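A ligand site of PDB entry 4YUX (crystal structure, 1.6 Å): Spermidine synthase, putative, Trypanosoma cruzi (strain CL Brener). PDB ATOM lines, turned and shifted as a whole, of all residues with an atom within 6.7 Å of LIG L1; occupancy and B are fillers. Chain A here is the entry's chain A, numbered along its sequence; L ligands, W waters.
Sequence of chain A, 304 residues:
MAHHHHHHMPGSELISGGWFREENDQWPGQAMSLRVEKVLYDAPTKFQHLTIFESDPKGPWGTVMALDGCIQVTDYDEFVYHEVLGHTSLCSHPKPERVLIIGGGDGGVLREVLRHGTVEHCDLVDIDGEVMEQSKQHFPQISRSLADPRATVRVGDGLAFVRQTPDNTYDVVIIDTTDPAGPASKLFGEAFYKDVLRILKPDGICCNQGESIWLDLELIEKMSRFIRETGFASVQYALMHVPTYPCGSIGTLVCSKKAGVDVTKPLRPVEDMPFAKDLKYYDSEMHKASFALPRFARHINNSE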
ATOM      1  N   GLU A  22      29.073  20.697 -30.481  1.00  0.00           N
ATOM      2  CA  GLU A  22      29.571  19.801 -29.418  1.00  0.00           C
ATOM      3  C   GLU A  22      31.045  19.482 -29.652  1.00  0.00           C
ATOM      4  O   GLU A  22      31.450  18.361 -29.960  1.00  0.00           O
ATOM      5  CB  GLU A  22      28.694  18.589 -29.334  1.00  0.00           C
ATOM      6  CG  GLU A  22      28.925  17.783 -28.057  1.00  0.00           C
ATOM      7  CD  GLU A  22      28.282  16.463 -28.078  1.00  0.00           C
ATOM      8  OE1 GLU A  22      28.296  15.797 -29.125  1.00  0.00           O
ATOM      9  OE2 GLU A  22      27.730  16.029 -27.066  1.00  0.00           O
ATOM     10  N   CYS A  70      28.644  18.675 -23.282  1.00  0.00           N
ATOM     11  CA  CYS A  70      28.277  17.335 -23.864  1.00  0.00           C
ATOM     12  C   CYS A  70      26.770  17.168 -23.773  1.00  0.00           C
ATOM     13  O   CYS A  70      26.168  17.233 -22.676  1.00  0.00           O
ATOM     14  CB  CYS A  70      28.936  16.245 -23.052  1.00  0.00           C
ATOM     15  SG  CYS A  70      30.757  16.329 -23.011  1.00  0.00           S
ATOM     16  N   ILE A  71      26.201  16.826 -24.906  1.00  0.00           N
ATOM     17  CA  ILE A  71      24.722  16.592 -24.990  1.00  0.00           C
ATOM     18  C   ILE A  71      24.381  15.396 -24.107  1.00  0.00           C
ATOM     19  O   ILE A  71      24.970  14.317 -24.246  1.00  0.00           O
ATOM     20  CB  ILE A  71      24.248  16.347 -26.439  1.00  0.00           C
ATOM     21  CG1 ILE A  71      24.434  17.593 -27.253  1.00  0.00           C
ATOM     22  CG2 ILE A  71      22.738  16.085 -26.378  1.00  0.00           C
ATOM     23  CD1 ILE A  71      24.352  17.307 -28.785  1.00  0.00           C
ATOM     24  N   GLN A  72      23.416  15.610 -23.217  1.00  0.00           N
ATOM     25  CA  GLN A  72      23.031  14.557 -22.222  1.00  0.00           C
ATOM     26  C   GLN A  72      21.707  13.888 -22.576  1.00  0.00           C
ATOM     27  O   GLN A  72      21.548  12.676 -22.391  1.00  0.00           O
ATOM     28  CB  GLN A  72      22.831  15.166 -20.859  1.00  0.00           C
ATOM     29  CG  GLN A  72      24.123  15.800 -20.261  1.00  0.00           C
ATOM     30  CD  GLN A  72      25.223  14.784 -20.034  1.00  0.00           C
ATOM     31  OE1 GLN A  72      25.074  13.862 -19.192  1.00  0.00           O
ATOM     32  NE2 GLN A  72      26.330  14.962 -20.709  1.00  0.00           N
ATOM     33  N   VAL A  73      20.733  14.745 -22.955  1.00  0.00           N
ATOM     34  CA  VAL A  73      19.404  14.245 -23.338  1.00  0.00           C
ATOM     35  C   VAL A  73      18.823  15.230 -24.384  1.00  0.00           C
ATOM     36  O   VAL A  73      19.151  16.374 -24.411  1.00  0.00           O
ATOM     37  CB  VAL A  73      18.364  14.091 -22.223  1.00  0.00           C
ATOM     38  CG1 VAL A  73      18.702  12.961 -21.189  1.00  0.00           C
ATOM     39  CG2 VAL A  73      18.193  15.415 -21.501  1.00  0.00           C
ATOM     40  N   THR A  74      18.015  14.656 -25.273  1.00  0.00           N
ATOM     41  CA  THR A  74      17.076  15.467 -26.079  1.00  0.00           C
ATOM     42  C   THR A  74      15.686  14.813 -25.959  1.00  0.00           C
ATOM     43  O   THR A  74      15.538  13.633 -25.655  1.00  0.00           O
ATOM     44  CB  THR A  74      17.446  15.533 -27.600  1.00  0.00           C
ATOM     45  OG1 THR A  74      17.033  14.310 -28.253  1.00  0.00           O
ATOM     46  CG2 THR A  74      18.933  15.776 -27.821  1.00  0.00           C
ATOM     47  N   ASP A  77      15.226  11.624 -28.558  1.00  0.00           N
ATOM     48  CA  ASP A  77      15.901  10.306 -28.492  1.00  0.00           C
ATOM     49  C   ASP A  77      16.218   9.887 -27.055  1.00  0.00           C
ATOM     50  O   ASP A  77      16.884   8.868 -26.877  1.00  0.00           O
ATOM     51  CB  ASP A  77      17.163  10.219 -29.399  1.00  0.00           C
ATOM     52  CG  ASP A  77      18.277  11.114 -28.916  1.00  0.00           C
ATOM     53  OD1 ASP A  77      18.076  11.777 -27.837  1.00  0.00           O
ATOM     54  OD2 ASP A  77      19.338  11.140 -29.564  1.00  0.00           O
ATOM     55  N   GLU A  78      15.759  10.587 -26.034  1.00  0.00           N
ATOM     56  CA  GLU A  78      16.121  10.215 -24.663  1.00  0.00           C
ATOM     57  C   GLU A  78      15.778   8.793 -24.291  1.00  0.00           C
ATOM     58  O   GLU A  78      16.450   8.171 -23.452  1.00  0.00           O
ATOM     59  CB  GLU A  78      15.664  11.188 -23.598  1.00  0.00           C
ATOM     60  CG  GLU A  78      14.140  11.328 -23.542  1.00  0.00           C
ATOM     61  CD  GLU A  78      13.402  10.330 -22.636  1.00  0.00           C
ATOM     62  OE1 GLU A  78      12.158  10.436 -22.568  1.00  0.00           O
ATOM     63  OE2 GLU A  78      13.974   9.461 -21.963  1.00  0.00           O
ATOM     64  N   TYR A  81      18.597   5.294 -24.384  1.00  0.00           N
ATOM     65  CA  TYR A  81      19.538   4.897 -23.392  1.00  0.00           C
ATOM     66  C   TYR A  81      18.833   4.615 -22.052  1.00  0.00           C
ATOM     67  O   TYR A  81      19.185   3.723 -21.312  1.00  0.00           O
ATOM     68  CB  TYR A  81      20.590   6.007 -23.353  1.00  0.00           C
ATOM     69  CG  TYR A  81      21.500   6.004 -22.143  1.00  0.00           C
ATOM     70  CD1 TYR A  81      21.149   6.633 -20.956  1.00  0.00           C
ATOM     71  CD2 TYR A  81      22.750   5.392 -22.226  1.00  0.00           C
ATOM     72  CE1 TYR A  81      22.056   6.678 -19.930  1.00  0.00           C
ATOM     73  CE2 TYR A  81      23.702   5.453 -21.238  1.00  0.00           C
ATOM     74  CZ  TYR A  81      23.351   6.102 -20.087  1.00  0.00           C
ATOM     75  OH  TYR A  81      24.235   6.187 -19.011  1.00  0.00           O
ATOM     76  N   HIS A  82      17.776   5.393 -21.784  1.00  0.00           N
ATOM     77  CA  HIS A  82      17.051   5.135 -20.533  1.00  0.00           C
ATOM     78  C   HIS A  82      16.360   3.778 -20.524  1.00  0.00           C
ATOM     79  O   HIS A  82      16.487   3.058 -19.534  1.00  0.00           O
ATOM     80  CB  HIS A  82      16.065   6.286 -20.329  1.00  0.00           C
ATOM     81  CG  HIS A  82      16.760   7.575 -20.118  1.00  0.00           C
ATOM     82  ND1 HIS A  82      16.217   8.813 -20.445  1.00  0.00           N
ATOM     83  CD2 HIS A  82      17.978   7.832 -19.577  1.00  0.00           C
ATOM     84  CE1 HIS A  82      17.090   9.768 -20.094  1.00  0.00           C
ATOM     85  NE2 HIS A  82      18.137   9.177 -19.553  1.00  0.00           N
ATOM     86  N   ASP A 176      24.894   5.696 -14.268  1.00  0.00           N
ATOM     87  CA  ASP A 176      24.488   6.570 -15.443  1.00  0.00           C
ATOM     88  C   ASP A 176      25.199   7.862 -15.291  1.00  0.00           C
ATOM     89  O   ASP A 176      24.669   8.873 -14.733  1.00  0.00           O
ATOM     90  CB  ASP A 176      22.927   6.772 -15.467  1.00  0.00           C
ATOM     91  CG  ASP A 176      22.561   7.838 -16.459  1.00  0.00           C
ATOM     92  OD1 ASP A 176      23.335   8.166 -17.329  1.00  0.00           O
ATOM     93  OD2 ASP A 176      21.450   8.363 -16.436  1.00  0.00           O
ATOM     94  N   THR A 177      26.438   7.911 -15.791  1.00  0.00           N
ATOM     95  CA  THR A 177      27.288   9.090 -15.541  1.00  0.00           C
ATOM     96  C   THR A 177      27.497   9.884 -16.842  1.00  0.00           C
ATOM     97  O   THR A 177      27.359   9.345 -17.972  1.00  0.00           O
ATOM     98  CB  THR A 177      28.658   8.681 -15.016  1.00  0.00           C
ATOM     99  OG1 THR A 177      29.312   7.849 -16.000  1.00  0.00           O
ATOM    100  CG2 THR A 177      28.520   7.865 -13.737  1.00  0.00           C
ATOM    101  N   THR A 178      27.966  11.097 -16.635  1.00  0.00           N
ATOM    102  CA  THR A 178      28.687  11.843 -17.715  1.00  0.00           C
ATOM    103  C   THR A 178      29.999  11.118 -18.104  1.00  0.00           C
ATOM    104  O   THR A 178      30.428  10.092 -17.541  1.00  0.00           O
ATOM    105  CB  THR A 178      29.038  13.249 -17.205  1.00  0.00           C
ATOM    106  OG1 THR A 178      29.554  13.132 -15.855  1.00  0.00           O
ATOM    107  CG2 THR A 178      27.816  14.187 -17.120  1.00  0.00           C
ATOM    108  N   ASP A 179      30.535  11.576 -19.215  1.00  0.00           N
ATOM    109  CA  ASP A 179      31.874  11.071 -19.694  1.00  0.00           C
ATOM    110  C   ASP A 179      32.950  11.367 -18.649  1.00  0.00           C
ATOM    111  O   ASP A 179      32.782  12.101 -17.644  1.00  0.00           O
ATOM    112  CB  ASP A 179      32.129  11.679 -21.087  1.00  0.00           C
ATOM    113  CG  ASP A 179      31.501  10.852 -22.255  1.00  0.00           C
ATOM    114  OD1 ASP A 179      31.014   9.689 -22.072  1.00  0.00           O
ATOM    115  OD2 ASP A 179      31.627  11.279 -23.388  1.00  0.00           O
ATOM    116  N   GLN A 209      27.534   3.528 -17.978  1.00  0.00           N
ATOM    117  CA  GLN A 209      27.597   4.327 -19.230  1.00  0.00           C
ATOM    118  C   GLN A 209      28.934   3.892 -19.831  1.00  0.00           C
ATOM    119  O   GLN A 209      29.996   4.290 -19.334  1.00  0.00           O
ATOM    120  CB  GLN A 209      27.443   5.791 -18.874  1.00  0.00           C
ATOM    121  CG  GLN A 209      27.323   6.743 -20.074  1.00  0.00           C
ATOM    122  CD  GLN A 209      28.652   7.076 -20.638  1.00  0.00           C
ATOM    123  OE1 GLN A 209      29.289   8.117 -20.213  1.00  0.00           O
ATOM    124  NE2 GLN A 209      29.045   6.398 -21.624  1.00  0.00           N
ATOM    125  N   MET A 240      23.952   0.331 -28.474  1.00  0.00           N
ATOM    126  CA  MET A 240      22.615   0.894 -28.802  1.00  0.00           C
ATOM    127  C   MET A 240      22.736   2.105 -29.692  1.00  0.00           C
ATOM    128  O   MET A 240      23.801   2.735 -29.790  1.00  0.00           O
ATOM    129  CB  MET A 240      21.825   1.222 -27.552  1.00  0.00           C
ATOM    130  CG  MET A 240      22.397   2.432 -26.755  1.00  0.00           C
ATOM    131  SD  MET A 240      21.964   2.530 -24.969  1.00  0.00           S
ATOM    132  CE  MET A 240      23.264   1.521 -24.233  1.00  0.00           C
ATOM    133  N   VAL A 242      22.051   5.815 -30.423  1.00  0.00           N
ATOM    134  CA  VAL A 242      21.698   7.098 -29.803  1.00  0.00           C
ATOM    135  C   VAL A 242      22.286   8.197 -30.667  1.00  0.00           C
ATOM    136  O   VAL A 242      23.490   8.472 -30.649  1.00  0.00           O
ATOM    137  CB  VAL A 242      22.206   7.196 -28.349  1.00  0.00           C
ATOM    138  CG1 VAL A 242      21.889   8.591 -27.808  1.00  0.00           C
ATOM    139  CG2 VAL A 242      21.614   6.111 -27.445  1.00  0.00           C
ATOM    140  N   PRO A 243      21.400   8.856 -31.437  1.00  0.00           N
ATOM    141  CA  PRO A 243      21.936   9.894 -32.422  1.00  0.00           C
ATOM    142  C   PRO A 243      22.772  10.996 -31.749  1.00  0.00           C
ATOM    143  O   PRO A 243      23.736  11.547 -32.346  1.00  0.00           O
ATOM    144  CB  PRO A 243      20.665  10.502 -32.960  1.00  0.00           C
ATOM    145  CG  PRO A 243      19.676   9.330 -33.028  1.00  0.00           C
ATOM    146  CD  PRO A 243      19.971   8.538 -31.683  1.00  0.00           C
ATOM    147  N   THR A 244      22.343  11.338 -30.505  1.00  0.00           N
ATOM    148  CA  THR A 244      22.995  12.467 -29.836  1.00  0.00           C
ATOM    149  C   THR A 244      24.075  12.153 -28.822  1.00  0.00           C
ATOM    150  O   THR A 244      24.361  12.974 -27.905  1.00  0.00           O
ATOM    151  CB  THR A 244      21.950  13.480 -29.273  1.00  0.00           C
ATOM    152  OG1 THR A 244      21.138  12.799 -28.351  1.00  0.00           O
ATOM    153  CG2 THR A 244      21.127  13.970 -30.461  1.00  0.00           C
ATOM    154  N   TYR A 245      24.706  10.998 -28.976  1.00  0.00           N
ATOM    155  CA  TYR A 245      25.957  10.754 -28.384  1.00  0.00           C
ATOM    156  C   TYR A 245      26.989  10.680 -29.476  1.00  0.00           C
ATOM    157  O   TYR A 245      26.729  10.192 -30.556  1.00  0.00           O
ATOM    158  CB  TYR A 245      25.893   9.440 -27.508  1.00  0.00           C
ATOM    159  CG  TYR A 245      27.148   9.171 -26.670  1.00  0.00           C
ATOM    160  CD1 TYR A 245      27.343   9.812 -25.401  1.00  0.00           C
ATOM    161  CD2 TYR A 245      28.163   8.316 -27.140  1.00  0.00           C
ATOM    162  CE1 TYR A 245      28.457   9.584 -24.649  1.00  0.00           C
ATOM    163  CE2 TYR A 245      29.309   8.120 -26.391  1.00  0.00           C
ATOM    164  CZ  TYR A 245      29.442   8.759 -25.136  1.00  0.00           C
ATOM    165  OH  TYR A 245      30.582   8.565 -24.369  1.00  0.00           O
ATOM    166  N   PRO A 246      28.213  11.127 -29.171  1.00  0.00           N
ATOM    167  CA  PRO A 246      29.178  11.169 -30.244  1.00  0.00           C
ATOM    168  C   PRO A 246      29.390   9.863 -31.018  1.00  0.00           C
ATOM    169  O   PRO A 246      29.596   8.823 -30.403  1.00  0.00           O
ATOM    170  CB  PRO A 246      30.490  11.643 -29.546  1.00  0.00           C
ATOM    171  CG  PRO A 246      29.952  12.465 -28.425  1.00  0.00           C
ATOM    172  CD  PRO A 246      28.659  11.813 -27.947  1.00  0.00           C
ATOM    173  N   ILE A 250      26.275   4.267 -28.265  1.00  0.00           N
ATOM    174  CA  ILE A 250      26.848   4.216 -26.946  1.00  0.00           C
ATOM    175  C   ILE A 250      26.552   2.805 -26.447  1.00  0.00           C
ATOM    176  O   ILE A 250      25.684   2.050 -27.025  1.00  0.00           O
ATOM    177  CB  ILE A 250      26.164   5.296 -26.036  1.00  0.00           C
ATOM    178  CG1 ILE A 250      26.890   5.512 -24.708  1.00  0.00           C
ATOM    179  CG2 ILE A 250      24.668   5.011 -25.922  1.00  0.00           C
ATOM    180  CD1 ILE A 250      26.332   6.656 -23.854  1.00  0.00           C
HETATM  181  C1  LIG L   1      26.129  11.131 -21.246  1.00  0.00           C
HETATM  182  C2  LIG L   1      25.753   9.890 -20.808  1.00  0.00           C
HETATM  183  C3  LIG L   1      25.563  11.657 -22.398  1.00  0.00           C
HETATM  184  C4  LIG L   1      24.834   9.135 -21.549  1.00  0.00           C
HETATM  185  C5  LIG L   1      24.620  10.911 -23.129  1.00  0.00           C
HETATM  186  C6  LIG L   1      24.296   9.663 -22.711  1.00  0.00           C
HETATM  187  C7  LIG L   1      22.885  11.200 -24.718  1.00  0.00           C
HETATM  188  C8  LIG L   1      22.034  10.196 -24.088  1.00  0.00           C
HETATM  189  N1  LIG L   1      24.058  11.509 -24.269  1.00  0.00           N
HETATM  190  N2  LIG L   1      22.334  11.892 -25.770  1.00  0.00           N
HETATM  191  S1  LIG L   1      23.110   8.763 -23.705  1.00  0.00           S
HETATM  192  C1  LG2 L   2      21.469  10.423 -19.619  1.00  0.00           C
HETATM  193  N1  LG2 L   2      20.554  10.169 -18.447  1.00  0.00           N
HETATM  194  C2  LG2 L   2      22.520  11.517 -19.391  1.00  0.00           C
HETATM  195  C3  LG2 L   2      23.540  11.216 -18.262  1.00  0.00           C
HETATM  196  S1  LG2 L   2      23.092  11.816 -16.640  1.00  0.00           S
HETATM  197  C4  LG2 L   2      22.725  13.555 -16.954  1.00  0.00           C
HETATM  198  C5  LG2 L   2      24.813  11.941 -15.990  1.00  0.00           C
HETATM  199  C6  LG2 L   2      24.836  12.359 -14.515  1.00  0.00           C
HETATM  200  O1  LG2 L   2      26.081  11.937 -13.974  1.00  0.00           O
HETATM  201  C7  LG2 L   2      26.290  12.852 -12.830  1.00  0.00           C
HETATM  202  C8  LG2 L   2      26.077  14.195 -13.508  1.00  0.00           C
HETATM  203  O2  LG2 L   2      25.862  15.259 -12.510  1.00  0.00           O
HETATM  204  C9  LG2 L   2      24.893  13.894 -14.444  1.00  0.00           C
HETATM  205  O3  LG2 L   2      23.656  14.453 -13.931  1.00  0.00           O
HETATM  206  N2  LG2 L   2      27.581  12.650 -12.174  1.00  0.00           N
HETATM  207  C10 LG2 L   2      28.843  13.018 -12.618  1.00  0.00           C
HETATM  208  N3  LG2 L   2      29.786  12.710 -11.772  1.00  0.00           N
HETATM  209  C11 LG2 L   2      29.164  12.121 -10.708  1.00  0.00           C
HETATM  210  C12 LG2 L   2      29.582  11.675  -9.456  1.00  0.00           C
HETATM  211  N4  LG2 L   2      30.946  11.724  -9.094  1.00  0.00           N
HETATM  212  C13 LG2 L   2      27.792  12.058 -10.940  1.00  0.00           C
HETATM  213  N5  LG2 L   2      26.871  11.596 -10.109  1.00  0.00           N
HETATM  214  C14 LG2 L   2      27.360  11.105  -8.940  1.00  0.00           C
HETATM  215  N6  LG2 L   2      28.673  11.147  -8.620  1.00  0.00           N
HETATM  216  O   HOH W   1      19.327  11.546 -25.561  1.00  0.00           O
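OG1 of Thr 244 is in hydrogen-bond range of N2 of LIG L1, 3.0 Å away.
The side-chain carboxylate of Asp 176 lies within salt-bridge range of a nitrogen (N1) of LG2 L2 (2.8 Å).
N1 of LIG L1 lies close to O of Gln 72.
N1 of LIG L1 sits close to O of Ile 71, 3.0 Å away.
A ring nitrogen (NE2) of His 82 is in hydrogen-bond range of a nitrogen (N1) of LG2 L2 (2.8 Å).
O of Thr 244 lies within hydrogen-bond range of N2 of LIG L1.
N of Thr 178 sits close to O1 of LG2 L2, 3.4 Å away.
The side-chain carboxylate (OE2) of Glu 22 lies within hydrogen-bond range of the backbone NH (N) of Ile 71 (2.8 Å).
OE1 of Gln 209 lies close to O of Thr 177 (3.2 Å).
The side-chain hydroxyl (OG1) of Thr 244 is in hydrogen-bond range of the side-chain carboxylate (OD2) of Asp 77, 2.7 Å away.
OD1 of Asp 179 lies within hydrogen-bond range of OH of Tyr 245, at 2.6 Å.
The side-chain amide oxygen (OE1) of Gln 209 sits close to the side-chain carboxylate (OD1) of Asp 179 (3.0 Å).
The side-chain carboxylate (OD1) of Asp 176 sits at hydrogen-bond distance from the side-chain hydroxyl (OH) of Tyr 81 (2.7 Å).
The backbone NH of Met 240 sits at hydrogen-bond distance from the backbone carbonyl oxygen of Ile 250.
The side-chain amide nitrogen (NE2) of Gln 72 is in hydrogen-bond range of the backbone carbonyl oxygen (O) of Cys 70, 3.0 Å away.
CG of Tyr 81 touches S1 of LIG L1 (3.6 Å).
O of Thr 177 touches C2 of LIG L1, at 3.3 Å.
Gln 209 touches LIG L1 (CG to C2, 3.6 Å).
CG1 of Val 242 touches N2 of LIG L1 (3.9 Å).
Tyr 245 touches LIG L1.
Ile 250 touches LIG L1 (CD1 to C4, 3.7 Å).
Hydrophobic or aromatic side chains within 4 Å of LIG L1: Tyr 81, Val 242, Tyr 245 and Ile 250.
Of the 22 residues printed, 9 come within 4 Å of LIG L1.
Water W1 lies within hydrogen-bond range of the side-chain carboxylate (OD1) of Asp 77 (2.6 Å), a nitrogen (N2) of LIG L1 (3.0 Å) and the backbone NH (N) of Thr 74 (3.4 Å).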
